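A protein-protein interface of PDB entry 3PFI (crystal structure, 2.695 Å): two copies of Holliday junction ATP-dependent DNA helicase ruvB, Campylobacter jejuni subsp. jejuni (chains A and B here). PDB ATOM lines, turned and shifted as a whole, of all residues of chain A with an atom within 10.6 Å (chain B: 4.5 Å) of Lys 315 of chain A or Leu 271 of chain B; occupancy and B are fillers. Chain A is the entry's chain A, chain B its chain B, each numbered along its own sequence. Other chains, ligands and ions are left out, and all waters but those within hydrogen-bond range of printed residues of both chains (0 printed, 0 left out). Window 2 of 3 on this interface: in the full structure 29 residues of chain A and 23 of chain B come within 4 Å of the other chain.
NH2 of Arg 267 of chain B lies within hydrogen-bond range of O of Leu 289 of chain B (3.2 Å).
The backbone NH of Arg 317 of chain A is in hydrogen-bond range of the backbone carbonyl oxygen of Ile 280 of chain A (2.8 Å).
O of Glu 270 of chain B lies within hydrogen-bond range of OG1 of Thr 273 of chain B (3.2 Å).
The side-chain hydroxyl (OG1) of Thr 313 of chain A lies within hydrogen-bond range of the backbone carbonyl oxygen (O) of Gly 316 of chain A.
Of the 11 printed residues of chain B, 4 touch a printed residue of chain A.
Hydrophobic or aromatic side chains of chain B that line the printed part of chain A: Leu 271.
Along chain B the printed residues that touch a printed residue of chain A span positions 267 to 288.
Of the 20 printed residues of chain A, 4 touch a printed residue of chain B.
Along chain A the printed residues that touch a printed residue of chain B span positions 313 to 317.
Among the printed residues, 5 pairs touch across the chains.
Among the printed residues, no Asp or Glu carboxylate lies within 4 Å of a Lys or Arg side-chain nitrogen of the other chain.
Tyr 268 of chain A touches none of the printed residues of chain B.
Glu 311 of chain A touches none of the printed residues of chain B.
Of the printed residues of chain B, Thr 313 of chain A touches Arg 267.
Of the printed residues of chain B, Lys 315 of chain A touches Leu 271 and Ala 288.
Printed residues of chain B within 4 Å of Arg 317 of chain A: Arg 267 (3.9 Å).
Printed residues of chain A within 4 Å of Arg 267 of chain B: Thr 313 (3.9 Å) and Arg 317 (3.9 Å).
Of the printed residues of chain A, Glu 270 of chain B touches Ala 314 (3.8 Å).
Leu 271 of chain B touches just one residue of chain A: Lys 315 (3.4 Å).
No residue of chain A comes within 4 Å of Leu 272 of chain B.
No residue of chain A comes within 4 Å of Thr 273 of chain B.
No residue of chain A comes within 4 Å of Ala 275 of chain B.
Arg 267 of chain B touches Thr 313 of chain A.
CB of Ala 314 of chain A touches OE1 of Glu 270 of chain B, 3.8 Å away.
Lys 315 of chain A touches Leu 271 of chain B (CG to CD2, 3.4 Å).
Lys 315 of chain A touches Ala 288 of chain B.
Arg 317 of chain A touches Arg 267 of chain B (NH2 to NH1, 3.9 Å).
Positions printed for both chains: 268 and 272.
Of the 5 pairs that touch across the chains among the printed residues, none has its exchanged pair printed and touching as well.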
ATOM      1  N   TYR A 268     -11.731  -5.026 -15.565  1.00  0.00           N
ATOM      2  CA  TYR A 268     -11.894  -3.685 -15.023  1.00  0.00           C
ATOM      3  C   TYR A 268     -11.142  -3.545 -13.700  1.00  0.00           C
ATOM      4  O   TYR A 268     -10.395  -2.591 -13.501  1.00  0.00           O
ATOM      5  CB  TYR A 268     -13.380  -3.363 -14.823  1.00  0.00           C
ATOM      6  CG  TYR A 268     -13.638  -1.947 -14.345  1.00  0.00           C
ATOM      7  CD1 TYR A 268     -14.039  -0.956 -15.230  1.00  0.00           C
ATOM      8  CD2 TYR A 268     -13.458  -1.596 -13.010  1.00  0.00           C
ATOM      9  CE1 TYR A 268     -14.268   0.341 -14.796  1.00  0.00           C
ATOM     10  CE2 TYR A 268     -13.682  -0.306 -12.571  1.00  0.00           C
ATOM     11  CZ  TYR A 268     -14.085   0.658 -13.467  1.00  0.00           C
ATOM     12  OH  TYR A 268     -14.310   1.941 -13.030  1.00  0.00           O
ATOM     13  N   LEU A 272      -7.761  -1.081 -12.824  1.00  0.00           N
ATOM     14  CA  LEU A 272      -7.658  -0.125 -11.725  1.00  0.00           C
ATOM     15  C   LEU A 272      -6.692  -0.609 -10.654  1.00  0.00           C
ATOM     16  O   LEU A 272      -5.932   0.180 -10.098  1.00  0.00           O
ATOM     17  CB  LEU A 272      -9.021   0.139 -11.081  1.00  0.00           C
ATOM     18  CG  LEU A 272     -10.026   1.000 -11.844  1.00  0.00           C
ATOM     19  CD1 LEU A 272     -10.429   0.368 -13.164  1.00  0.00           C
ATOM     20  CD2 LEU A 272     -11.242   1.231 -10.969  1.00  0.00           C
ATOM     21  N   LYS A 276      -2.039   2.258  -9.362  1.00  0.00           N
ATOM     22  CA  LYS A 276      -1.983   2.398  -7.915  1.00  0.00           C
ATOM     23  C   LYS A 276      -3.141   3.281  -7.475  1.00  0.00           C
ATOM     24  O   LYS A 276      -3.937   3.712  -8.312  1.00  0.00           O
ATOM     25  CB  LYS A 276      -0.640   2.993  -7.484  1.00  0.00           C
ATOM     26  CG  LYS A 276       0.586   2.159  -7.883  1.00  0.00           C
ATOM     27  CD  LYS A 276       0.784   2.079  -9.399  1.00  0.00           C
ATOM     28  CE  LYS A 276       2.028   1.289  -9.767  1.00  0.00           C
ATOM     29  NZ  LYS A 276       1.945  -0.125  -9.311  1.00  0.00           N
ATOM     30  N   GLN A 277      -3.252   3.546  -6.175  1.00  0.00           N
ATOM     31  CA  GLN A 277      -4.330   4.398  -5.669  1.00  0.00           C
ATOM     32  C   GLN A 277      -4.294   5.769  -6.344  1.00  0.00           C
ATOM     33  O   GLN A 277      -4.093   6.799  -5.702  1.00  0.00           O
ATOM     34  CB  GLN A 277      -4.267   4.533  -4.143  1.00  0.00           C
ATOM     35  CG  GLN A 277      -4.601   3.246  -3.397  1.00  0.00           C
ATOM     36  CD  GLN A 277      -4.616   3.423  -1.889  1.00  0.00           C
ATOM     37  OE1 GLN A 277      -4.148   4.436  -1.364  1.00  0.00           O
ATOM     38  NE2 GLN A 277      -5.153   2.433  -1.186  1.00  0.00           N
ATOM     39  N   LYS A 278      -4.493   5.748  -7.658  1.00  0.00           N
ATOM     40  CA  LYS A 278      -4.506   6.940  -8.485  1.00  0.00           C
ATOM     41  C   LYS A 278      -5.695   6.776  -9.422  1.00  0.00           C
ATOM     42  O   LYS A 278      -5.765   5.805 -10.175  1.00  0.00           O
ATOM     43  CB  LYS A 278      -3.192   7.077  -9.258  1.00  0.00           C
ATOM     44  CG  LYS A 278      -1.973   7.261  -8.349  1.00  0.00           C
ATOM     45  CD  LYS A 278      -0.666   7.476  -9.115  1.00  0.00           C
ATOM     46  CE  LYS A 278      -0.196   6.232  -9.863  1.00  0.00           C
ATOM     47  NZ  LYS A 278      -1.113   5.812 -10.957  1.00  0.00           N
ATOM     48  N   PRO A 279      -6.637   7.728  -9.378  1.00  0.00           N
ATOM     49  CA  PRO A 279      -7.864   7.628 -10.166  1.00  0.00           C
ATOM     50  C   PRO A 279      -7.695   7.663 -11.684  1.00  0.00           C
ATOM     51  O   PRO A 279      -6.898   8.438 -12.209  1.00  0.00           O
ATOM     52  CB  PRO A 279      -8.678   8.836  -9.695  1.00  0.00           C
ATOM     53  CG  PRO A 279      -7.664   9.822  -9.243  1.00  0.00           C
ATOM     54  CD  PRO A 279      -6.539   9.016  -8.668  1.00  0.00           C
ATOM     55  N   ILE A 280      -8.450   6.810 -12.368  1.00  0.00           N
ATOM     56  CA  ILE A 280      -8.439   6.736 -13.823  1.00  0.00           C
ATOM     57  C   ILE A 280      -9.799   7.206 -14.331  1.00  0.00           C
ATOM     58  O   ILE A 280     -10.837   6.738 -13.858  1.00  0.00           O
ATOM     59  CB  ILE A 280      -8.181   5.300 -14.315  1.00  0.00           C
ATOM     60  CG1 ILE A 280      -6.853   4.776 -13.767  1.00  0.00           C
ATOM     61  CG2 ILE A 280      -8.165   5.249 -15.830  1.00  0.00           C
ATOM     62  CD1 ILE A 280      -6.502   3.389 -14.256  1.00  0.00           C
ATOM     63  N   GLY A 281      -9.794   8.134 -15.283  1.00  0.00           N
ATOM     64  CA  GLY A 281     -11.036   8.659 -15.841  1.00  0.00           C
ATOM     65  C   GLY A 281     -11.542   7.826 -17.002  1.00  0.00           C
ATOM     66  O   GLY A 281     -10.766   7.130 -17.658  1.00  0.00           O
ATOM     67  N   LEU A 282     -12.846   7.895 -17.254  1.00  0.00           N
ATOM     68  CA  LEU A 282     -13.456   7.156 -18.356  1.00  0.00           C
ATOM     69  C   LEU A 282     -12.595   7.214 -19.608  1.00  0.00           C
ATOM     70  O   LEU A 282     -12.304   6.186 -20.216  1.00  0.00           O
ATOM     71  CB  LEU A 282     -14.840   7.714 -18.679  1.00  0.00           C
ATOM     72  CG  LEU A 282     -15.958   7.429 -17.681  1.00  0.00           C
ATOM     73  CD1 LEU A 282     -17.197   8.229 -18.038  1.00  0.00           C
ATOM     74  CD2 LEU A 282     -16.259   5.938 -17.652  1.00  0.00           C
ATOM     75  N   ALA A 283     -12.197   8.425 -19.989  1.00  0.00           N
ATOM     76  CA  ALA A 283     -11.363   8.632 -21.169  1.00  0.00           C
ATOM     77  C   ALA A 283     -10.311   7.535 -21.273  1.00  0.00           C
ATOM     78  O   ALA A 283     -10.179   6.883 -22.309  1.00  0.00           O
ATOM     79  CB  ALA A 283     -10.701  10.003 -21.115  1.00  0.00           C
ATOM     80  N   SER A 284      -9.572   7.332 -20.186  1.00  0.00           N
ATOM     81  CA  SER A 284      -8.530   6.314 -20.139  1.00  0.00           C
ATOM     82  C   SER A 284      -9.142   4.919 -20.100  1.00  0.00           C
ATOM     83  O   SER A 284      -8.864   4.088 -20.964  1.00  0.00           O
ATOM     84  CB  SER A 284      -7.638   6.521 -18.913  1.00  0.00           C
ATOM     85  OG  SER A 284      -7.023   7.796 -18.936  1.00  0.00           O
ATOM     86  N   ILE A 285      -9.980   4.674 -19.096  1.00  0.00           N
ATOM     87  CA  ILE A 285     -10.629   3.374 -18.926  1.00  0.00           C
ATOM     88  C   ILE A 285     -11.272   2.893 -20.219  1.00  0.00           C
ATOM     89  O   ILE A 285     -10.997   1.786 -20.682  1.00  0.00           O
ATOM     90  CB  ILE A 285     -11.714   3.417 -17.827  1.00  0.00           C
ATOM     91  CG1 ILE A 285     -11.088   3.720 -16.466  1.00  0.00           C
ATOM     92  CG2 ILE A 285     -12.460   2.095 -17.765  1.00  0.00           C
ATOM     93  CD1 ILE A 285     -12.077   3.718 -15.329  1.00  0.00           C
ATOM     94  N   GLU A 311     -14.830   3.103  -6.624  1.00  0.00           N
ATOM     95  CA  GLU A 311     -15.440   4.382  -6.270  1.00  0.00           C
ATOM     96  C   GLU A 311     -15.150   5.447  -7.323  1.00  0.00           C
ATOM     97  O   GLU A 311     -14.081   5.449  -7.935  1.00  0.00           O
ATOM     98  CB  GLU A 311     -14.937   4.854  -4.904  1.00  0.00           C
ATOM     99  CG  GLU A 311     -15.300   3.923  -3.755  1.00  0.00           C
ATOM    100  CD  GLU A 311     -14.845   4.443  -2.403  1.00  0.00           C
ATOM    101  OE1 GLU A 311     -14.095   5.443  -2.364  1.00  0.00           O
ATOM    102  OE2 GLU A 311     -15.237   3.843  -1.379  1.00  0.00           O
ATOM    103  N   ARG A 312     -16.111   6.344  -7.529  1.00  0.00           N
ATOM    104  CA  ARG A 312     -15.972   7.434  -8.494  1.00  0.00           C
ATOM    105  C   ARG A 312     -15.543   8.709  -7.777  1.00  0.00           C
ATOM    106  O   ARG A 312     -16.384   9.494  -7.340  1.00  0.00           O
ATOM    107  CB  ARG A 312     -17.293   7.673  -9.230  1.00  0.00           C
ATOM    108  CG  ARG A 312     -17.791   6.475 -10.016  1.00  0.00           C
ATOM    109  CD  ARG A 312     -19.110   6.771 -10.716  1.00  0.00           C
ATOM    110  NE  ARG A 312     -19.599   5.613 -11.462  1.00  0.00           N
ATOM    111  CZ  ARG A 312     -20.737   5.586 -12.151  1.00  0.00           C
ATOM    112  NH1 ARG A 312     -21.096   4.484 -12.798  1.00  0.00           N
ATOM    113  NH2 ARG A 312     -21.517   6.656 -12.197  1.00  0.00           N
ATOM    114  N   THR A 313     -14.233   8.911  -7.661  1.00  0.00           N
ATOM    115  CA  THR A 313     -13.696  10.090  -6.985  1.00  0.00           C
ATOM    116  C   THR A 313     -13.918  11.346  -7.819  1.00  0.00           C
ATOM    117  O   THR A 313     -14.457  11.286  -8.923  1.00  0.00           O
ATOM    118  CB  THR A 313     -12.185   9.942  -6.699  1.00  0.00           C
ATOM    119  OG1 THR A 313     -11.456   9.907  -7.932  1.00  0.00           O
ATOM    120  CG2 THR A 313     -11.911   8.674  -5.899  1.00  0.00           C
ATOM    121  N   ALA A 314     -13.494  12.484  -7.279  1.00  0.00           N
ATOM    122  CA  ALA A 314     -13.647  13.767  -7.954  1.00  0.00           C
ATOM    123  C   ALA A 314     -12.953  13.808  -9.315  1.00  0.00           C
ATOM    124  O   ALA A 314     -13.412  14.502 -10.223  1.00  0.00           O
ATOM    125  CB  ALA A 314     -13.123  14.885  -7.065  1.00  0.00           C
ATOM    126  N   LYS A 315     -11.853  13.072  -9.458  1.00  0.00           N
ATOM    127  CA  LYS A 315     -11.107  13.054 -10.714  1.00  0.00           C
ATOM    128  C   LYS A 315     -10.741  11.642 -11.171  1.00  0.00           C
ATOM    129  O   LYS A 315      -9.561  11.315 -11.291  1.00  0.00           O
ATOM    130  CB  LYS A 315      -9.830  13.891 -10.580  1.00  0.00           C
ATOM    131  CG  LYS A 315     -10.080  15.351 -10.226  1.00  0.00           C
ATOM    132  CD  LYS A 315      -8.790  16.169 -10.188  1.00  0.00           C
ATOM    133  CE  LYS A 315      -7.820  15.678  -9.120  1.00  0.00           C
ATOM    134  NZ  LYS A 315      -6.601  16.530  -9.047  1.00  0.00           N
ATOM    135  N   GLY A 316     -11.749  10.813 -11.430  1.00  0.00           N
ATOM    136  CA  GLY A 316     -11.521   9.442 -11.898  1.00  0.00           C
ATOM    137  C   GLY A 316     -12.023   8.369 -10.950  1.00  0.00           C
ATOM    138  O   GLY A 316     -12.790   8.653 -10.028  1.00  0.00           O
ATOM    139  N   ARG A 317     -11.592   7.130 -11.186  1.00  0.00           N
ATOM    140  CA  ARG A 317     -12.004   5.984 -10.370  1.00  0.00           C
ATOM    141  C   ARG A 317     -10.848   5.296  -9.645  1.00  0.00           C
ATOM    142  O   ARG A 317      -9.700   5.373 -10.072  1.00  0.00           O
ATOM    143  CB  ARG A 317     -12.745   4.951 -11.229  1.00  0.00           C
ATOM    144  CG  ARG A 317     -14.155   5.361 -11.648  1.00  0.00           C
ATOM    145  CD  ARG A 317     -14.176   6.562 -12.580  1.00  0.00           C
ATOM    146  NE  ARG A 317     -15.540   7.021 -12.833  1.00  0.00           N
ATOM    147  CZ  ARG A 317     -16.338   6.534 -13.776  1.00  0.00           C
ATOM    148  NH1 ARG A 317     -15.923   5.557 -14.570  1.00  0.00           N
ATOM    149  NH2 ARG A 317     -17.561   7.022 -13.921  1.00  0.00           N
ATOM    150  N   ILE A 318     -11.174   4.615  -8.548  1.00  0.00           N
ATOM    151  CA  ILE A 318     -10.186   3.897  -7.745  1.00  0.00           C
ATOM    152  C   ILE A 318     -10.776   2.596  -7.196  1.00  0.00           C
ATOM    153  O   ILE A 318     -11.986   2.491  -6.997  1.00  0.00           O
ATOM    154  CB  ILE A 318      -9.703   4.752  -6.563  1.00  0.00           C
ATOM    155  CG1 ILE A 318     -10.866   5.070  -5.620  1.00  0.00           C
ATOM    156  CG2 ILE A 318      -9.065   6.034  -7.065  1.00  0.00           C
ATOM    157  CD1 ILE A 318     -10.477   5.936  -4.445  1.00  0.00           C
ATOM    158  N   ARG B 267     -19.453  16.056  -8.756  1.00  0.00           N
ATOM    159  CA  ARG B 267     -18.033  15.930  -9.071  1.00  0.00           C
ATOM    160  C   ARG B 267     -17.488  17.284  -9.502  1.00  0.00           C
ATOM    161  O   ARG B 267     -16.439  17.718  -9.025  1.00  0.00           O
ATOM    162  CB  ARG B 267     -17.777  14.885 -10.158  1.00  0.00           C
ATOM    163  CG  ARG B 267     -18.235  13.486  -9.788  1.00  0.00           C
ATOM    164  CD  ARG B 267     -17.666  12.432 -10.726  1.00  0.00           C
ATOM    165  NE  ARG B 267     -17.869  12.746 -12.138  1.00  0.00           N
ATOM    166  CZ  ARG B 267     -17.513  11.939 -13.136  1.00  0.00           C
ATOM    167  NH1 ARG B 267     -16.958  10.760 -12.880  1.00  0.00           N
ATOM    168  NH2 ARG B 267     -17.725  12.301 -14.393  1.00  0.00           N
ATOM    169  N   TYR B 268     -18.212  17.951 -10.395  1.00  0.00           N
ATOM    170  CA  TYR B 268     -17.814  19.262 -10.883  1.00  0.00           C
ATOM    171  C   TYR B 268     -17.538  20.218  -9.719  1.00  0.00           C
ATOM    172  O   TYR B 268     -16.502  20.881  -9.687  1.00  0.00           O
ATOM    173  CB  TYR B 268     -18.908  19.841 -11.786  1.00  0.00           C
ATOM    174  CG  TYR B 268     -18.542  21.159 -12.439  1.00  0.00           C
ATOM    175  CD1 TYR B 268     -17.897  21.192 -13.666  1.00  0.00           C
ATOM    176  CD2 TYR B 268     -18.848  22.368 -11.833  1.00  0.00           C
ATOM    177  CE1 TYR B 268     -17.561  22.391 -14.270  1.00  0.00           C
ATOM    178  CE2 TYR B 268     -18.515  23.573 -12.432  1.00  0.00           C
ATOM    179  CZ  TYR B 268     -17.872  23.576 -13.652  1.00  0.00           C
ATOM    180  OH  TYR B 268     -17.537  24.768 -14.254  1.00  0.00           O
ATOM    181  N   LEU B 269     -18.469  20.280  -8.768  1.00  0.00           N
ATOM    182  CA  LEU B 269     -18.332  21.164  -7.608  1.00  0.00           C
ATOM    183  C   LEU B 269     -17.211  20.733  -6.661  1.00  0.00           C
ATOM    184  O   LEU B 269     -16.570  21.574  -6.036  1.00  0.00           O
ATOM    185  CB  LEU B 269     -19.663  21.280  -6.856  1.00  0.00           C
ATOM    186  CG  LEU B 269     -20.723  22.135  -7.556  1.00  0.00           C
ATOM    187  CD1 LEU B 269     -22.113  21.939  -6.950  1.00  0.00           C
ATOM    188  CD2 LEU B 269     -20.309  23.600  -7.522  1.00  0.00           C
ATOM    189  N   GLU B 270     -16.989  19.427  -6.551  1.00  0.00           N
ATOM    190  CA  GLU B 270     -15.915  18.909  -5.717  1.00  0.00           C
ATOM    191  C   GLU B 270     -14.581  19.269  -6.357  1.00  0.00           C
ATOM    192  O   GLU B 270     -13.587  19.504  -5.671  1.00  0.00           O
ATOM    193  CB  GLU B 270     -16.025  17.390  -5.559  1.00  0.00           C
ATOM    194  CG  GLU B 270     -17.236  16.922  -4.763  1.00  0.00           C
ATOM    195  CD  GLU B 270     -17.272  15.413  -4.578  1.00  0.00           C
ATOM    196  OE1 GLU B 270     -16.259  14.747  -4.885  1.00  0.00           O
ATOM    197  OE2 GLU B 270     -18.309  14.893  -4.118  1.00  0.00           O
ATOM    198  N   LEU B 271     -14.580  19.315  -7.684  1.00  0.00           N
ATOM    199  CA  LEU B 271     -13.395  19.644  -8.458  1.00  0.00           C
ATOM    200  C   LEU B 271     -13.037  21.118  -8.253  1.00  0.00           C
ATOM    201  O   LEU B 271     -11.894  21.446  -7.939  1.00  0.00           O
ATOM    202  CB  LEU B 271     -13.660  19.329  -9.938  1.00  0.00           C
ATOM    203  CG  LEU B 271     -12.528  19.409 -10.964  1.00  0.00           C
ATOM    204  CD1 LEU B 271     -12.092  20.845 -11.202  1.00  0.00           C
ATOM    205  CD2 LEU B 271     -11.355  18.534 -10.537  1.00  0.00           C
ATOM    206  N   LEU B 272     -14.023  21.999  -8.415  1.00  0.00           N
ATOM    207  CA  LEU B 272     -13.810  23.441  -8.241  1.00  0.00           C
ATOM    208  C   LEU B 272     -13.571  23.858  -6.789  1.00  0.00           C
ATOM    209  O   LEU B 272     -12.703  24.691  -6.522  1.00  0.00           O
ATOM    210  CB  LEU B 272     -14.976  24.247  -8.829  1.00  0.00           C
ATOM    211  CG  LEU B 272     -14.972  24.465 -10.348  1.00  0.00           C
ATOM    212  CD1 LEU B 272     -14.785  23.171 -11.116  1.00  0.00           C
ATOM    213  CD2 LEU B 272     -16.251  25.169 -10.780  1.00  0.00           C
ATOM    214  N   THR B 273     -14.335  23.297  -5.854  1.00  0.00           N
ATOM    215  CA  THR B 273     -14.160  23.643  -4.442  1.00  0.00           C
ATOM    216  C   THR B 273     -12.753  23.287  -3.974  1.00  0.00           C
ATOM    217  O   THR B 273     -12.102  24.076  -3.297  1.00  0.00           O
ATOM    218  CB  THR B 273     -15.196  22.952  -3.532  1.00  0.00           C
ATOM    219  OG1 THR B 273     -15.178  21.539  -3.768  1.00  0.00           O
ATOM    220  CG2 THR B 273     -16.593  23.495  -3.801  1.00  0.00           C
ATOM    221  N   ALA B 274     -12.287  22.102  -4.356  1.00  0.00           N
ATOM    222  CA  ALA B 274     -10.951  21.649  -3.997  1.00  0.00           C
ATOM    223  C   ALA B 274      -9.900  22.630  -4.501  1.00  0.00           C
ATOM    224  O   ALA B 274      -8.818  22.748  -3.914  1.00  0.00           O
ATOM    225  CB  ALA B 274     -10.694  20.260  -4.571  1.00  0.00           C
ATOM    226  N   ALA B 275     -10.233  23.347  -5.576  1.00  0.00           N
ATOM    227  CA  ALA B 275      -9.315  24.314  -6.190  1.00  0.00           C
ATOM    228  C   ALA B 275      -9.155  25.632  -5.420  1.00  0.00           C
ATOM    229  O   ALA B 275      -8.450  26.532  -5.881  1.00  0.00           O
ATOM    230  CB  ALA B 275      -9.738  24.594  -7.622  1.00  0.00           C
ATOM    231  N   ALA B 288     -10.962  16.125 -16.474  1.00  0.00           N
ATOM    232  CA  ALA B 288     -11.241  15.637 -15.121  1.00  0.00           C
ATOM    233  C   ALA B 288     -12.586  14.918 -14.995  1.00  0.00           C
ATOM    234  O   ALA B 288     -12.701  13.934 -14.267  1.00  0.00           O
ATOM    235  CB  ALA B 288     -11.172  16.791 -14.127  1.00  0.00           C
ATOM    236  N   LEU B 289     -13.599  15.416 -15.697  1.00  0.00           N
ATOM    237  CA  LEU B 289     -14.935  14.826 -15.648  1.00  0.00           C
ATOM    238  C   LEU B 289     -15.229  13.941 -16.856  1.00  0.00           C
ATOM    239  O   LEU B 289     -16.350  13.453 -17.007  1.00  0.00           O
ATOM    240  CB  LEU B 289     -15.993  15.925 -15.566  1.00  0.00           C
ATOM    241  CG  LEU B 289     -16.034  16.750 -14.282  1.00  0.00           C
ATOM    242  CD1 LEU B 289     -14.665  17.293 -13.906  1.00  0.00           C
ATOM    243  CD2 LEU B 289     -17.034  17.873 -14.457  1.00  0.00           C
